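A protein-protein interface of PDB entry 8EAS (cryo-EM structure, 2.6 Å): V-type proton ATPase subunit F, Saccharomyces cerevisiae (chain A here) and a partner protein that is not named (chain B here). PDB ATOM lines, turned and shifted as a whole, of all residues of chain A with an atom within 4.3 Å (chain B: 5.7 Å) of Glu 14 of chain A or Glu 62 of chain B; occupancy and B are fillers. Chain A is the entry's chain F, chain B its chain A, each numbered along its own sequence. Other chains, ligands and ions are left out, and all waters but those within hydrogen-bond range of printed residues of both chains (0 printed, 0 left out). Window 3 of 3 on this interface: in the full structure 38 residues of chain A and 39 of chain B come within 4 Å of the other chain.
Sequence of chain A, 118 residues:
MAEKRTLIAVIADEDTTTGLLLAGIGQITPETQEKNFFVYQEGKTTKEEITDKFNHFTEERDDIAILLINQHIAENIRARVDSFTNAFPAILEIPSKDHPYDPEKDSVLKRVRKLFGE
The side-chain carboxylate of Glu 14 of chain A lies within hydrogen-bond range of the backbone NH of Glu 62 of chain B (3.0 Å).
NE1 of Trp 65 of chain B lies within hydrogen-bond range of OG1 of Thr 18 of chain A (2.9 Å).
NE1 of Trp 65 of chain B sits close to O of Gly 61 of chain B (3.2 Å).
The backbone carbonyl oxygen of Asp 13 of chain A is in hydrogen-bond range of the side-chain hydroxyl of Thr 17 of chain A, at 2.8 Å.
O of Glu 14 of chain A lies within hydrogen-bond range of OG1 of Thr 18 of chain A, 3.0 Å away.
Among the printed residues, merely in contact across the chains: Glu 14 of chain A with Gly 61 of chain B (3.0 Å), Glu 14 of chain A with Trp 65 of chain B (3.0 Å), Thr 17 of chain A with Trp 65 of chain B (3.6 Å), Thr 18 of chain A with Tyr 60 of chain B (3.8 Å) and Thr 18 of chain A with Gly 61 of chain B (3.5 Å).
Asp 13 of chain A touches none of the printed residues of chain B.
Of chain B, only Gly 61 (3.0 Å), Glu 62 (3.0 Å) and Trp 65 (3.0 Å) come within 4 Å of Glu 14 of chain A.
Of the printed residues of chain B, Thr 17 of chain A touches Trp 65 (3.6 Å).
Printed residues of chain B within 4 Å of Thr 18 of chain A: Tyr 60, Gly 61 and Trp 65.
Of the printed residues of chain A, Tyr 60 of chain B touches Thr 18.
Of the printed residues of chain A, Gly 61 of chain B touches Glu 14 and Thr 18.
Of chain A, only Glu 14 comes within 4 Å of Glu 62 of chain B.
Printed residues of chain A within 4 Å of Trp 65 of chain B: Glu 14, Thr 17 and Thr 18.
The nearest residue of chain B that does not touch Glu 14 of chain A is Asn 59 of chain B (4.6 Å).
The nearest printed residue of chain B that does not touch Thr 17 of chain A is Glu 62 of chain B (7.2 Å).
Along chain A the printed residues that touch a printed residue of chain B span positions 14 to 18.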
ATOM      1  N   ASP A  13     -29.512  17.695  -3.905  1.00  0.00           N
ATOM      2  CA  ASP A  13     -30.171  18.135  -2.686  1.00  0.00           C
ATOM      3  C   ASP A  13     -29.501  19.414  -2.190  1.00  0.00           C
ATOM      4  O   ASP A  13     -28.701  20.038  -2.890  1.00  0.00           O
ATOM      5  CB  ASP A  13     -30.169  17.027  -1.637  1.00  0.00           C
ATOM      6  CG  ASP A  13     -28.798  16.445  -1.403  1.00  0.00           C
ATOM      7  OD1 ASP A  13     -27.986  16.456  -2.341  1.00  0.00           O
ATOM      8  OD2 ASP A  13     -28.530  15.970  -0.279  1.00  0.00           O
ATOM      9  N   GLU A  14     -29.833  19.820  -0.968  1.00  0.00           N
ATOM     10  CA  GLU A  14     -29.417  21.127  -0.471  1.00  0.00           C
ATOM     11  C   GLU A  14     -27.916  21.162  -0.195  1.00  0.00           C
ATOM     12  O   GLU A  14     -27.217  22.088  -0.621  1.00  0.00           O
ATOM     13  CB  GLU A  14     -30.245  21.465   0.772  1.00  0.00           C
ATOM     14  CG  GLU A  14     -30.141  22.878   1.316  1.00  0.00           C
ATOM     15  CD  GLU A  14     -28.955  23.088   2.226  1.00  0.00           C
ATOM     16  OE1 GLU A  14     -28.518  22.117   2.876  1.00  0.00           O
ATOM     17  OE2 GLU A  14     -28.483  24.234   2.320  1.00  0.00           O
ATOM     18  N   ASP A  15     -27.395  20.144   0.491  1.00  0.00           N
ATOM     19  CA  ASP A  15     -25.974  20.137   0.833  1.00  0.00           C
ATOM     20  C   ASP A  15     -25.102  19.927  -0.396  1.00  0.00           C
ATOM     21  O   ASP A  15     -24.031  20.532  -0.516  1.00  0.00           O
ATOM     22  CB  ASP A  15     -25.698  19.064   1.879  1.00  0.00           C
ATOM     23  CG  ASP A  15     -26.612  19.181   3.076  1.00  0.00           C
ATOM     24  OD1 ASP A  15     -26.310  19.990   3.978  1.00  0.00           O
ATOM     25  OD2 ASP A  15     -27.640  18.470   3.110  1.00  0.00           O
ATOM     26  N   THR A  16     -25.537  19.067  -1.317  1.00  0.00           N
ATOM     27  CA  THR A  16     -24.778  18.868  -2.546  1.00  0.00           C
ATOM     28  C   THR A  16     -24.783  20.127  -3.398  1.00  0.00           C
ATOM     29  O   THR A  16     -23.779  20.457  -4.034  1.00  0.00           O
ATOM     30  CB  THR A  16     -25.340  17.691  -3.335  1.00  0.00           C
ATOM     31  OG1 THR A  16     -25.372  16.530  -2.498  1.00  0.00           O
ATOM     32  CG2 THR A  16     -24.478  17.405  -4.548  1.00  0.00           C
ATOM     33  N   THR A  17     -25.909  20.840  -3.428  1.00  0.00           N
ATOM     34  CA  THR A  17     -25.950  22.113  -4.137  1.00  0.00           C
ATOM     35  C   THR A  17     -25.004  23.123  -3.509  1.00  0.00           C
ATOM     36  O   THR A  17     -24.304  23.849  -4.220  1.00  0.00           O
ATOM     37  CB  THR A  17     -27.375  22.660  -4.163  1.00  0.00           C
ATOM     38  OG1 THR A  17     -28.192  21.823  -4.987  1.00  0.00           O
ATOM     39  CG2 THR A  17     -27.394  24.072  -4.711  1.00  0.00           C
ATOM     40  N   THR A  18     -24.965  23.184  -2.175  1.00  0.00           N
ATOM     41  CA  THR A  18     -24.019  24.078  -1.514  1.00  0.00           C
ATOM     42  C   THR A  18     -22.588  23.719  -1.882  1.00  0.00           C
ATOM     43  O   THR A  18     -21.772  24.598  -2.180  1.00  0.00           O
ATOM     44  CB  THR A  18     -24.201  24.021   0.000  1.00  0.00           C
ATOM     45  OG1 THR A  18     -25.528  24.430   0.342  1.00  0.00           O
ATOM     46  CG2 THR A  18     -23.206  24.929   0.687  1.00  0.00           C
ATOM     47  N   TYR A  40     -33.366  19.522  -5.128  1.00  0.00           N
ATOM     48  CA  TYR A  40     -34.257  18.444  -4.732  1.00  0.00           C
ATOM     49  C   TYR A  40     -34.393  18.413  -3.219  1.00  0.00           C
ATOM     50  O   TYR A  40     -33.395  18.457  -2.495  1.00  0.00           O
ATOM     51  CB  TYR A  40     -33.723  17.114  -5.252  1.00  0.00           C
ATOM     52  CG  TYR A  40     -34.342  15.880  -4.640  1.00  0.00           C
ATOM     53  CD1 TYR A  40     -35.511  15.337  -5.151  1.00  0.00           C
ATOM     54  CD2 TYR A  40     -33.740  15.239  -3.566  1.00  0.00           C
ATOM     55  CE1 TYR A  40     -36.070  14.204  -4.598  1.00  0.00           C
ATOM     56  CE2 TYR A  40     -34.290  14.107  -3.009  1.00  0.00           C
ATOM     57  CZ  TYR A  40     -35.456  13.594  -3.530  1.00  0.00           C
ATOM     58  OH  TYR A  40     -36.010  12.462  -2.977  1.00  0.00           O
ATOM     59  N   ASN B  59     -26.801  28.071   9.675  1.00  0.00           N
ATOM     60  CA  ASN B  59     -26.551  27.086   8.640  1.00  0.00           C
ATOM     61  C   ASN B  59     -25.866  27.778   7.475  1.00  0.00           C
ATOM     62  O   ASN B  59     -26.154  28.937   7.170  1.00  0.00           O
ATOM     63  CB  ASN B  59     -27.861  26.426   8.195  1.00  0.00           C
ATOM     64  CG  ASN B  59     -27.646  25.255   7.273  1.00  0.00           C
ATOM     65  OD1 ASN B  59     -26.522  24.923   6.920  1.00  0.00           O
ATOM     66  ND2 ASN B  59     -28.736  24.621   6.869  1.00  0.00           N
ATOM     67  N   TYR B  60     -24.947  27.063   6.832  1.00  0.00           N
ATOM     68  CA  TYR B  60     -24.300  27.527   5.608  1.00  0.00           C
ATOM     69  C   TYR B  60     -24.902  26.736   4.457  1.00  0.00           C
ATOM     70  O   TYR B  60     -24.496  25.606   4.183  1.00  0.00           O
ATOM     71  CB  TYR B  60     -22.788  27.364   5.684  1.00  0.00           C
ATOM     72  CG  TYR B  60     -22.151  28.362   6.612  1.00  0.00           C
ATOM     73  CD1 TYR B  60     -21.925  29.666   6.210  1.00  0.00           C
ATOM     74  CD2 TYR B  60     -21.795  28.005   7.900  1.00  0.00           C
ATOM     75  CE1 TYR B  60     -21.359  30.579   7.060  1.00  0.00           C
ATOM     76  CE2 TYR B  60     -21.231  28.912   8.755  1.00  0.00           C
ATOM     77  CZ  TYR B  60     -21.011  30.196   8.332  1.00  0.00           C
ATOM     78  OH  TYR B  60     -20.441  31.100   9.189  1.00  0.00           O
ATOM     79  N   GLY B  61     -25.866  27.342   3.776  1.00  0.00           N
ATOM     80  CA  GLY B  61     -26.665  26.626   2.807  1.00  0.00           C
ATOM     81  C   GLY B  61     -27.547  27.530   1.977  1.00  0.00           C
ATOM     82  O   GLY B  61     -27.086  28.553   1.471  1.00  0.00           O
ATOM     83  N   GLU B  62     -28.817  27.150   1.822  1.00  0.00           N
ATOM     84  CA  GLU B  62     -29.725  27.875   0.938  1.00  0.00           C
ATOM     85  C   GLU B  62     -29.899  29.330   1.348  1.00  0.00           C
ATOM     86  O   GLU B  62     -30.310  30.157   0.529  1.00  0.00           O
ATOM     87  CB  GLU B  62     -31.080  27.174   0.901  1.00  0.00           C
ATOM     88  CG  GLU B  62     -31.815  27.191   2.226  1.00  0.00           C
ATOM     89  CD  GLU B  62     -33.121  26.433   2.173  1.00  0.00           C
ATOM     90  OE1 GLU B  62     -33.437  25.877   1.101  1.00  0.00           O
ATOM     91  OE2 GLU B  62     -33.828  26.393   3.200  1.00  0.00           O
ATOM     92  N   ASP B  63     -29.605  29.665   2.604  1.00  0.00           N
ATOM     93  CA  ASP B  63     -29.697  31.053   3.037  1.00  0.00           C
ATOM     94  C   ASP B  63     -28.744  31.944   2.259  1.00  0.00           C
ATOM     95  O   ASP B  63     -28.998  33.143   2.102  1.00  0.00           O
ATOM     96  CB  ASP B  63     -29.397  31.151   4.528  1.00  0.00           C
ATOM     97  CG  ASP B  63     -30.506  30.592   5.376  1.00  0.00           C
ATOM     98  OD1 ASP B  63     -30.203  30.032   6.449  1.00  0.00           O
ATOM     99  OD2 ASP B  63     -31.680  30.715   4.975  1.00  0.00           O
ATOM    100  N   TYR B  64     -27.649  31.376   1.767  1.00  0.00           N
ATOM    101  CA  TYR B  64     -26.601  32.128   1.103  1.00  0.00           C
ATOM    102  C   TYR B  64     -26.566  31.917  -0.398  1.00  0.00           C
ATOM    103  O   TYR B  64     -25.738  32.539  -1.069  1.00  0.00           O
ATOM    104  CB  TYR B  64     -25.238  31.739   1.673  1.00  0.00           C
ATOM    105  CG  TYR B  64     -25.032  32.099   3.116  1.00  0.00           C
ATOM    106  CD1 TYR B  64     -24.749  33.397   3.496  1.00  0.00           C
ATOM    107  CD2 TYR B  64     -25.115  31.133   4.102  1.00  0.00           C
ATOM    108  CE1 TYR B  64     -24.548  33.717   4.805  1.00  0.00           C
ATOM    109  CE2 TYR B  64     -24.918  31.447   5.416  1.00  0.00           C
ATOM    110  CZ  TYR B  64     -24.637  32.740   5.764  1.00  0.00           C
ATOM    111  OH  TYR B  64     -24.442  33.066   7.078  1.00  0.00           O
ATOM    112  N   TRP B  65     -27.408  31.046  -0.938  1.00  0.00           N
ATOM    113  CA  TRP B  65     -27.343  30.742  -2.357  1.00  0.00           C
ATOM    114  C   TRP B  65     -27.712  31.964  -3.173  1.00  0.00           C
ATOM    115  O   TRP B  65     -28.790  32.540  -3.003  1.00  0.00           O
ATOM    116  CB  TRP B  65     -28.269  29.585  -2.694  1.00  0.00           C
ATOM    117  CG  TRP B  65     -27.817  28.298  -2.134  1.00  0.00           C
ATOM    118  CD1 TRP B  65     -26.625  28.038  -1.534  1.00  0.00           C
ATOM    119  CD2 TRP B  65     -28.547  27.079  -2.125  1.00  0.00           C
ATOM    120  NE1 TRP B  65     -26.571  26.729  -1.141  1.00  0.00           N
ATOM    121  CE2 TRP B  65     -27.743  26.117  -1.495  1.00  0.00           C
ATOM    122  CE3 TRP B  65     -29.812  26.706  -2.578  1.00  0.00           C
ATOM    123  CZ2 TRP B  65     -28.159  24.810  -1.312  1.00  0.00           C
ATOM    124  CZ3 TRP B  65     -30.221  25.412  -2.396  1.00  0.00           C
ATOM    125  CH2 TRP B  65     -29.400  24.476  -1.770  1.00  0.00           C
